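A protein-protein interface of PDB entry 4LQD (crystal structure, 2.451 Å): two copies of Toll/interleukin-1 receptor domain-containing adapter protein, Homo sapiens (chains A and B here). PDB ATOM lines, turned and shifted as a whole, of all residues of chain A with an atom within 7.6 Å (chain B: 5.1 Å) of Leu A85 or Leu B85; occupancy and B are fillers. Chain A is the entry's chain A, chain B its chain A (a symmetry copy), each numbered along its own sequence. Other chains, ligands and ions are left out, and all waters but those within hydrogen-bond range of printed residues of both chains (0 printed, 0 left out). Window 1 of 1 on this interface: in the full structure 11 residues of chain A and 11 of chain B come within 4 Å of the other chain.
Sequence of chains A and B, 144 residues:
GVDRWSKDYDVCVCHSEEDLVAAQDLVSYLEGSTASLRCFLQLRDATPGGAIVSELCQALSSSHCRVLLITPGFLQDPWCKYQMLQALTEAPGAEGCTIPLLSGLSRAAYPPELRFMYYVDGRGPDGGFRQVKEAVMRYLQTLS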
ATOM      1  N   LEU A  68      17.606  28.485 -18.513  1.00  0.00           N
ATOM      2  CA  LEU A  68      18.914  28.641 -17.883  1.00  0.00           C
ATOM      3  C   LEU A  68      18.810  29.711 -16.794  1.00  0.00           C
ATOM      4  O   LEU A  68      18.615  30.900 -17.092  1.00  0.00           O
ATOM      5  CB  LEU A  68      19.981  29.006 -18.921  1.00  0.00           C
ATOM      6  CG  LEU A  68      19.987  28.139 -20.187  1.00  0.00           C
ATOM      7  CD1 LEU A  68      21.064  28.559 -21.179  1.00  0.00           C
ATOM      8  CD2 LEU A  68      20.154  26.682 -19.822  1.00  0.00           C
ATOM      9  N   PHE A  74      25.897  30.514 -11.276  1.00  0.00           N
ATOM     10  CA  PHE A  74      25.936  29.898 -12.596  1.00  0.00           C
ATOM     11  C   PHE A  74      27.195  30.331 -13.346  1.00  0.00           C
ATOM     12  O   PHE A  74      27.880  29.505 -13.941  1.00  0.00           O
ATOM     13  CB  PHE A  74      24.671  30.275 -13.377  1.00  0.00           C
ATOM     14  CG  PHE A  74      24.490  29.537 -14.684  1.00  0.00           C
ATOM     15  CD1 PHE A  74      23.617  28.454 -14.768  1.00  0.00           C
ATOM     16  CD2 PHE A  74      25.144  29.956 -15.837  1.00  0.00           C
ATOM     17  CE1 PHE A  74      23.421  27.790 -15.966  1.00  0.00           C
ATOM     18  CE2 PHE A  74      24.953  29.293 -17.045  1.00  0.00           C
ATOM     19  CZ  PHE A  74      24.092  28.210 -17.109  1.00  0.00           C
ATOM     20  N   TRP A  79      31.076  24.281 -15.556  1.00  0.00           N
ATOM     21  CA  TRP A  79      30.127  23.265 -16.009  1.00  0.00           C
ATOM     22  C   TRP A  79      28.783  23.897 -16.418  1.00  0.00           C
ATOM     23  O   TRP A  79      28.209  23.530 -17.454  1.00  0.00           O
ATOM     24  CB  TRP A  79      29.934  22.203 -14.921  1.00  0.00           C
ATOM     25  CG  TRP A  79      29.110  21.024 -15.354  1.00  0.00           C
ATOM     26  CD1 TRP A  79      27.909  20.627 -14.830  1.00  0.00           C
ATOM     27  CD2 TRP A  79      29.414  20.095 -16.408  1.00  0.00           C
ATOM     28  NE1 TRP A  79      27.453  19.508 -15.494  1.00  0.00           N
ATOM     29  CE2 TRP A  79      28.360  19.160 -16.461  1.00  0.00           C
ATOM     30  CE3 TRP A  79      30.478  19.961 -17.306  1.00  0.00           C
ATOM     31  CZ2 TRP A  79      28.338  18.101 -17.384  1.00  0.00           C
ATOM     32  CZ3 TRP A  79      30.456  18.907 -18.221  1.00  0.00           C
ATOM     33  CH2 TRP A  79      29.391  17.995 -18.255  1.00  0.00           C
ATOM     34  N   CME A  80      28.311  24.869 -15.637  1.00  0.00           N
ATOM     35  CA  CME A  80      27.124  25.590 -15.992  1.00  0.00           C
ATOM     36  CB  CME A  80      26.825  26.709 -15.014  1.00  0.00           C
ATOM     37  SG  CME A  80      26.125  26.042 -13.524  1.00  0.00           S
ATOM     38  SD  CME A  80      24.570  24.840 -14.048  1.00  0.00           S
ATOM     39  CE  CME A  80      25.110  23.123 -13.958  1.00  0.00           C
ATOM     40  CZ  CME A  80      25.431  22.747 -12.483  1.00  0.00           C
ATOM     41  OH  CME A  80      25.364  21.313 -12.327  1.00  0.00           O
ATOM     42  C   CME A  80      27.284  26.180 -17.369  1.00  0.00           C
ATOM     43  O   CME A  80      26.380  26.021 -18.227  1.00  0.00           O
ATOM     44  N   LYS A  81      28.441  26.791 -17.621  1.00  0.00           N
ATOM     45  CA  LYS A  81      28.680  27.427 -18.911  1.00  0.00           C
ATOM     46  C   LYS A  81      28.566  26.364 -19.983  1.00  0.00           C
ATOM     47  O   LYS A  81      27.880  26.560 -21.002  1.00  0.00           O
ATOM     48  CB  LYS A  81      30.050  28.108 -18.952  1.00  0.00           C
ATOM     49  CG  LYS A  81      30.437  28.814 -17.638  1.00  0.00           C
ATOM     50  CD  LYS A  81      29.842  30.218 -17.511  1.00  0.00           C
ATOM     51  CE  LYS A  81      30.653  31.252 -18.298  1.00  0.00           C
ATOM     52  NZ  LYS A  81      31.957  31.556 -17.642  1.00  0.00           N
ATOM     53  N   TYR A  82      29.165  25.206 -19.705  1.00  0.00           N
ATOM     54  CA  TYR A  82      29.118  24.111 -20.656  1.00  0.00           C
ATOM     55  C   TYR A  82      27.665  23.718 -20.915  1.00  0.00           C
ATOM     56  O   TYR A  82      27.256  23.583 -22.075  1.00  0.00           O
ATOM     57  CB  TYR A  82      29.930  22.920 -20.156  1.00  0.00           C
ATOM     58  CG  TYR A  82      29.982  21.786 -21.145  1.00  0.00           C
ATOM     59  CD1 TYR A  82      30.693  21.909 -22.335  1.00  0.00           C
ATOM     60  CD2 TYR A  82      29.315  20.595 -20.899  1.00  0.00           C
ATOM     61  CE1 TYR A  82      30.741  20.864 -23.253  1.00  0.00           C
ATOM     62  CE2 TYR A  82      29.363  19.543 -21.801  1.00  0.00           C
ATOM     63  CZ  TYR A  82      30.070  19.685 -22.975  1.00  0.00           C
ATOM     64  OH  TYR A  82      30.102  18.639 -23.861  1.00  0.00           O
ATOM     65  N   GLN A  83      26.874  23.595 -19.847  1.00  0.00           N
ATOM     66  CA  GLN A  83      25.463  23.244 -20.016  1.00  0.00           C
ATOM     67  C   GLN A  83      24.772  24.259 -20.899  1.00  0.00           C
ATOM     68  O   GLN A  83      23.982  23.872 -21.768  1.00  0.00           O
ATOM     69  CB  GLN A  83      24.731  23.140 -18.675  1.00  0.00           C
ATOM     70  CG  GLN A  83      25.063  21.887 -17.880  1.00  0.00           C
ATOM     71  CD  GLN A  83      24.970  20.617 -18.710  1.00  0.00           C
ATOM     72  OE1 GLN A  83      25.845  19.758 -18.639  1.00  0.00           O
ATOM     73  NE2 GLN A  83      23.908  20.489 -19.492  1.00  0.00           N
ATOM     74  N   MET A  84      25.100  25.542 -20.718  1.00  0.00           N
ATOM     75  CA  MET A  84      24.487  26.576 -21.554  1.00  0.00           C
ATOM     76  C   MET A  84      24.738  26.244 -23.020  1.00  0.00           C
ATOM     77  O   MET A  84      23.787  26.190 -23.816  1.00  0.00           O
ATOM     78  CB  MET A  84      25.021  27.962 -21.200  1.00  0.00           C
ATOM     79  CG  MET A  84      24.501  29.092 -22.076  1.00  0.00           C
ATOM     80  SD  MET A  84      24.968  30.704 -21.375  1.00  0.00           S
ATOM     81  CE  MET A  84      24.669  31.728 -22.817  1.00  0.00           C
ATOM     82  N   LEU A  85      25.998  25.934 -23.348  1.00  0.00           N
ATOM     83  CA  LEU A  85      26.369  25.526 -24.711  1.00  0.00           C
ATOM     84  C   LEU A  85      25.569  24.326 -25.205  1.00  0.00           C
ATOM     85  O   LEU A  85      25.139  24.290 -26.360  1.00  0.00           O
ATOM     86  CB  LEU A  85      27.857  25.187 -24.787  1.00  0.00           C
ATOM     87  CG  LEU A  85      28.753  26.161 -25.538  1.00  0.00           C
ATOM     88  CD1 LEU A  85      28.772  27.471 -24.806  1.00  0.00           C
ATOM     89  CD2 LEU A  85      30.156  25.602 -25.665  1.00  0.00           C
ATOM     90  N   GLN A  86      25.366  23.346 -24.328  1.00  0.00           N
ATOM     91  CA  GLN A  86      24.622  22.148 -24.708  1.00  0.00           C
ATOM     92  C   GLN A  86      23.146  22.468 -24.924  1.00  0.00           C
ATOM     93  O   GLN A  86      22.457  21.776 -25.673  1.00  0.00           O
ATOM     94  CB  GLN A  86      24.774  21.054 -23.644  1.00  0.00           C
ATOM     95  CG  GLN A  86      26.212  20.588 -23.435  1.00  0.00           C
ATOM     96  CD  GLN A  86      26.719  19.755 -24.592  1.00  0.00           C
ATOM     97  OE1 GLN A  86      27.479  20.234 -25.444  1.00  0.00           O
ATOM     98  NE2 GLN A  86      26.295  18.497 -24.635  1.00  0.00           N
ATOM     99  N   ALA A  87      22.659  23.517 -24.267  1.00  0.00           N
ATOM    100  CA  ALA A  87      21.252  23.858 -24.391  1.00  0.00           C
ATOM    101  C   ALA A  87      20.988  24.505 -25.747  1.00  0.00           C
ATOM    102  O   ALA A  87      19.893  24.391 -26.289  1.00  0.00           O
ATOM    103  CB  ALA A  87      20.818  24.779 -23.249  1.00  0.00           C
ATOM    104  N   LEU A  88      22.002  25.162 -26.301  1.00  0.00           N
ATOM    105  CA  LEU A  88      21.857  25.852 -27.581  1.00  0.00           C
ATOM    106  C   LEU A  88      22.315  25.024 -28.792  1.00  0.00           C
ATOM    107  O   LEU A  88      22.668  25.583 -29.829  1.00  0.00           O
ATOM    108  CB  LEU A  88      22.622  27.174 -27.534  1.00  0.00           C
ATOM    109  CG  LEU A  88      22.212  28.043 -26.345  1.00  0.00           C
ATOM    110  CD1 LEU A  88      23.120  29.241 -26.191  1.00  0.00           C
ATOM    111  CD2 LEU A  88      20.777  28.500 -26.505  1.00  0.00           C
ATOM    112  N   THR A  89      22.314  23.699 -28.663  1.00  0.00           N
ATOM    113  CA  THR A  89      22.550  22.831 -29.815  1.00  0.00           C
ATOM    114  C   THR A  89      21.284  22.047 -30.117  1.00  0.00           C
ATOM    115  O   THR A  89      20.871  21.189 -29.331  1.00  0.00           O
ATOM    116  CB  THR A  89      23.721  21.831 -29.606  1.00  0.00           C
ATOM    117  OG1 THR A  89      23.232  20.489 -29.714  1.00  0.00           O
ATOM    118  CG2 THR A  89      24.365  22.004 -28.253  1.00  0.00           C
ATOM    119  N   GLU A  90      20.675  22.353 -31.258  1.00  0.00           N
ATOM    120  CA  GLU A  90      19.433  21.714 -31.675  1.00  0.00           C
ATOM    121  C   GLU A  90      19.659  20.751 -32.841  1.00  0.00           C
ATOM    122  O   GLU A  90      19.886  19.556 -32.639  1.00  0.00           O
ATOM    123  CB  GLU A  90      18.404  22.778 -32.053  1.00  0.00           C
ATOM    124  CG  GLU A  90      19.013  23.973 -32.772  1.00  0.00           C
ATOM    125  CD  GLU A  90      18.018  25.092 -32.998  1.00  0.00           C
ATOM    126  OE1 GLU A  90      16.829  24.911 -32.658  1.00  0.00           O
ATOM    127  OE2 GLU A  90      18.425  26.155 -33.514  1.00  0.00           O
ATOM    128  N   GLU A 113      27.456  36.795 -25.532  1.00  0.00           N
ATOM    129  CA  GLU A 113      26.639  36.139 -26.555  1.00  0.00           C
ATOM    130  C   GLU A 113      25.215  36.697 -26.552  1.00  0.00           C
ATOM    131  O   GLU A 113      24.600  36.903 -27.609  1.00  0.00           O
ATOM    132  CB  GLU A 113      26.583  34.620 -26.330  1.00  0.00           C
ATOM    133  CG  GLU A 113      27.919  33.906 -26.284  1.00  0.00           C
ATOM    134  CD  GLU A 113      28.476  33.772 -24.883  1.00  0.00           C
ATOM    135  OE1 GLU A 113      29.384  32.937 -24.673  1.00  0.00           O
ATOM    136  OE2 GLU A 113      28.026  34.513 -23.993  1.00  0.00           O
ATOM    137  N   LEU A 114      24.696  36.947 -25.353  1.00  0.00           N
ATOM    138  CA  LEU A 114      23.312  37.347 -25.208  1.00  0.00           C
ATOM    139  C   LEU A 114      23.025  38.720 -25.834  1.00  0.00           C
ATOM    140  O   LEU A 114      21.860  39.079 -26.015  1.00  0.00           O
ATOM    141  CB  LEU A 114      22.919  37.321 -23.731  1.00  0.00           C
ATOM    142  CG  LEU A 114      23.044  35.929 -23.092  1.00  0.00           C
ATOM    143  CD1 LEU A 114      22.628  35.951 -21.639  1.00  0.00           C
ATOM    144  CD2 LEU A 114      22.231  34.907 -23.843  1.00  0.00           C
ATOM    145  N   MET A 117      21.164  37.448 -28.675  1.00  0.00           N
ATOM    146  CA  MET A 117      20.195  36.390 -28.448  1.00  0.00           C
ATOM    147  C   MET A 117      19.032  36.847 -27.572  1.00  0.00           C
ATOM    148  O   MET A 117      19.106  37.866 -26.894  1.00  0.00           O
ATOM    149  CB  MET A 117      20.884  35.186 -27.811  1.00  0.00           C
ATOM    150  CG  MET A 117      21.991  34.611 -28.667  1.00  0.00           C
ATOM    151  SD  MET A 117      23.037  33.481 -27.738  1.00  0.00           S
ATOM    152  CE  MET A 117      21.802  32.387 -27.060  1.00  0.00           C
ATOM    153  N   LYS B  81      32.438  35.767 -29.750  1.00  0.00           N
ATOM    154  CA  LYS B  81      31.917  34.778 -28.815  1.00  0.00           C
ATOM    155  C   LYS B  81      30.684  34.155 -29.434  1.00  0.00           C
ATOM    156  O   LYS B  81      30.540  32.919 -29.458  1.00  0.00           O
ATOM    157  CB  LYS B  81      31.593  35.409 -27.458  1.00  0.00           C
ATOM    158  CG  LYS B  81      32.615  36.468 -27.001  1.00  0.00           C
ATOM    159  CD  LYS B  81      33.849  35.863 -26.327  1.00  0.00           C
ATOM    160  CE  LYS B  81      33.577  35.503 -24.862  1.00  0.00           C
ATOM    161  NZ  LYS B  81      33.483  36.714 -23.998  1.00  0.00           N
ATOM    162  N   TYR B  82      29.843  35.009 -30.017  1.00  0.00           N
ATOM    163  CA  TYR B  82      28.630  34.526 -30.649  1.00  0.00           C
ATOM    164  C   TYR B  82      28.987  33.547 -31.766  1.00  0.00           C
ATOM    165  O   TYR B  82      28.415  32.453 -31.839  1.00  0.00           O
ATOM    166  CB  TYR B  82      27.793  35.685 -31.180  1.00  0.00           C
ATOM    167  CG  TYR B  82      26.482  35.243 -31.773  1.00  0.00           C
ATOM    168  CD1 TYR B  82      25.467  34.739 -30.965  1.00  0.00           C
ATOM    169  CD2 TYR B  82      26.257  35.317 -33.140  1.00  0.00           C
ATOM    170  CE1 TYR B  82      24.254  34.326 -31.510  1.00  0.00           C
ATOM    171  CE2 TYR B  82      25.050  34.917 -33.694  1.00  0.00           C
ATOM    172  CZ  TYR B  82      24.059  34.419 -32.877  1.00  0.00           C
ATOM    173  OH  TYR B  82      22.873  34.020 -33.440  1.00  0.00           O
ATOM    174  N   GLN B  83      29.970  33.910 -32.593  1.00  0.00           N
ATOM    175  CA  GLN B  83      30.386  33.016 -33.674  1.00  0.00           C
ATOM    176  C   GLN B  83      30.822  31.681 -33.112  1.00  0.00           C
ATOM    177  O   GLN B  83      30.470  30.638 -33.677  1.00  0.00           O
ATOM    178  CB  GLN B  83      31.515  33.616 -34.517  1.00  0.00           C
ATOM    179  CG  GLN B  83      31.068  34.725 -35.456  1.00  0.00           C
ATOM    180  CD  GLN B  83      29.846  34.348 -36.278  1.00  0.00           C
ATOM    181  OE1 GLN B  83      28.917  35.140 -36.416  1.00  0.00           O
ATOM    182  NE2 GLN B  83      29.845  33.144 -36.831  1.00  0.00           N
ATOM    183  N   MET B  84      31.536  31.704 -31.982  1.00  0.00           N
ATOM    184  CA  MET B  84      31.972  30.447 -31.370  1.00  0.00           C
ATOM    185  C   MET B  84      30.753  29.567 -31.119  1.00  0.00           C
ATOM    186  O   MET B  84      30.730  28.401 -31.547  1.00  0.00           O
ATOM    187  CB  MET B  84      32.748  30.701 -30.079  1.00  0.00           C
ATOM    188  CG  MET B  84      33.168  29.447 -29.327  1.00  0.00           C
ATOM    189  SD  MET B  84      34.325  29.868 -27.988  1.00  0.00           S
ATOM    190  CE  MET B  84      34.224  28.344 -27.049  1.00  0.00           C
ATOM    191  N   LEU B  85      29.715  30.154 -30.514  1.00  0.00           N
ATOM    192  CA  LEU B  85      28.450  29.444 -30.273  1.00  0.00           C
ATOM    193  C   LEU B  85      27.841  28.877 -31.550  1.00  0.00           C
ATOM    194  O   LEU B  85      27.342  27.750 -31.562  1.00  0.00           O
ATOM    195  CB  LEU B  85      27.430  30.368 -29.610  1.00  0.00           C
ATOM    196  CG  LEU B  85      27.099  30.101 -28.149  1.00  0.00           C
ATOM    197  CD1 LEU B  85      28.323  30.349 -27.318  1.00  0.00           C
ATOM    198  CD2 LEU B  85      25.957  30.988 -27.693  1.00  0.00           C
ATOM    199  N   GLN B  86      27.886  29.659 -32.626  1.00  0.00           N
ATOM    200  CA  GLN B  86      27.317  29.214 -33.895  1.00  0.00           C
ATOM    201  C   GLN B  86      28.143  28.080 -34.495  1.00  0.00           C
ATOM    202  O   GLN B  86      27.629  27.264 -35.259  1.00  0.00           O
ATOM    203  CB  GLN B  86      27.222  30.379 -34.887  1.00  0.00           C
ATOM    204  CG  GLN B  86      26.323  31.520 -34.419  1.00  0.00           C
ATOM    205  CD  GLN B  86      24.855  31.151 -34.469  1.00  0.00           C
ATOM    206  OE1 GLN B  86      24.236  30.847 -33.441  1.00  0.00           O
ATOM    207  NE2 GLN B  86      24.289  31.168 -35.670  1.00  0.00           N
ATOM    208  N   ALA B  87      29.427  28.028 -34.151  1.00  0.00           N
ATOM    209  CA  ALA B  87      30.287  27.002 -34.716  1.00  0.00           C
ATOM    210  C   ALA B  87      29.992  25.656 -34.061  1.00  0.00           C
ATOM    211  O   ALA B  87      30.162  24.611 -34.681  1.00  0.00           O
ATOM    212  CB  ALA B  87      31.759  27.382 -34.552  1.00  0.00           C
ATOM    213  N   LEU B  88      29.528  25.688 -32.815  1.00  0.00           N
ATOM    214  CA  LEU B  88      29.245  24.461 -32.074  1.00  0.00           C
ATOM    215  C   LEU B  88      27.774  24.020 -32.136  1.00  0.00           C
ATOM    216  O   LEU B  88      27.300  23.310 -31.250  1.00  0.00           O
ATOM    217  CB  LEU B  88      29.676  24.637 -30.619  1.00  0.00           C
ATOM    218  CG  LEU B  88      31.133  25.080 -30.491  1.00  0.00           C
ATOM    219  CD1 LEU B  88      31.480  25.454 -29.069  1.00  0.00           C
ATOM    220  CD2 LEU B  88      32.055  23.981 -30.976  1.00  0.00           C
ATOM    221  N   THR B  89      27.052  24.441 -33.173  1.00  0.00           N
ATOM    222  CA  THR B  89      25.707  23.920 -33.413  1.00  0.00           C
ATOM    223  C   THR B  89      25.706  23.117 -34.703  1.00  0.00           C
ATOM    224  O   THR B  89      25.879  23.673 -35.793  1.00  0.00           O
ATOM    225  CB  THR B  89      24.624  25.030 -33.513  1.00  0.00           C
ATOM    226  OG1 THR B  89      24.001  24.978 -34.802  1.00  0.00           O
ATOM    227  CG2 THR B  89      25.215  26.403 -33.314  1.00  0.00           C
ATOM    228  N   GLU B 113      34.197  26.733 -20.866  1.00  0.00           N
ATOM    229  CA  GLU B 113      33.604  25.622 -21.615  1.00  0.00           C
ATOM    230  C   GLU B 113      34.680  24.629 -22.056  1.00  0.00           C
ATOM    231  O   GLU B 113      34.482  23.405 -22.019  1.00  0.00           O
ATOM    232  CB  GLU B 113      32.852  26.129 -22.855  1.00  0.00           C
ATOM    233  CG  GLU B 113      31.757  27.145 -22.599  1.00  0.00           C
ATOM    234  CD  GLU B 113      32.236  28.577 -22.697  1.00  0.00           C
ATOM    235  OE1 GLU B 113      31.389  29.489 -22.831  1.00  0.00           O
ATOM    236  OE2 GLU B 113      33.455  28.801 -22.621  1.00  0.00           O
ATOM    237  N   MET B 117      35.944  20.388 -23.433  1.00  0.00           N
ATOM    238  CA  MET B 117      35.945  20.233 -24.877  1.00  0.00           C
ATOM    239  C   MET B 117      37.353  20.084 -25.444  1.00  0.00           C
ATOM    240  O   MET B 117      38.342  20.395 -24.787  1.00  0.00           O
ATOM    241  CB  MET B 117      35.247  21.426 -25.525  1.00  0.00           C
ATOM    242  CG  MET B 117      33.808  21.585 -25.087  1.00  0.00           C
ATOM    243  SD  MET B 117      33.146  23.196 -25.533  1.00  0.00           S
ATOM    244  CE  MET B 117      33.536  23.232 -27.272  1.00  0.00           C
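Leu A85 touches just these residues of chain B: Leu B85 (3.8 Å), Leu B88 (3.7 Å), Glu B113 (3.7 Å) and Met B117 (3.8 Å).
Of the printed residues of chain B, Tyr A82 touches Met B117 (3.6 Å).
Of the printed residues of chain B, Met A117 touches Tyr B82 (3.6 Å) and Leu B85 (3.8 Å).
Of the printed residues of chain A, Glu B113 touches Leu A85.
Thr A89 touches none of the printed residues of chain B.
Lys A81 touches none of the printed residues of chain B.
The nearest printed residue of chain B that does not touch Leu A85 is Met B84 (5.1 Å).
Leu B85 touches its own counterpart, Leu A85.
Leu A85 touches Leu B88, and with the chains exchanged Leu A88 touches Leu B85.
Leu A85 touches Glu B113, and with the chains exchanged Glu A113 touches Leu B85.
Leu A85 touches Met B117, and with the chains exchanged Met A117 touches Leu B85.
Positions printed for both chains: 81, 82, 83, 84, 85, 86, 87, 88, 89, 113 and 117.
Of the 9 pairs that touch across the chains among the printed residues, 9 have their exchanged pair printed and touching as well.
OE1 of Gln B86 is in hydrogen-bond range of OH of Tyr B82.
The side-chain hydroxyl (OH) of Tyr A82 is in hydrogen-bond range of the side-chain amide oxygen (OE1) of Gln A86 (3.5 Å).
Of the 11 printed residues of chain B, 5 touch a printed residue of chain A.
Printed residues of chain A that touch a printed residue of chain B: Tyr A82, Leu A85, Leu A88, Glu A113 and Met A117.
Hydrophobic or aromatic side chains of chain A that line the printed part of chain B: Tyr A82, Leu A85, Leu A88 and Met A117.
Among the printed residues, 9 pairs touch across the chains.
Among the printed residues, merely in contact across the chains: Tyr A82 with Met B117, Leu A85 with Leu B85, Leu A85 with Leu B88, Leu A85 with Glu B113, Leu A85 with Met B117, Leu A88 with Leu B85, Glu A113 with Leu B85, Met A117 with Tyr B82 and Met A117 with Leu B85.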
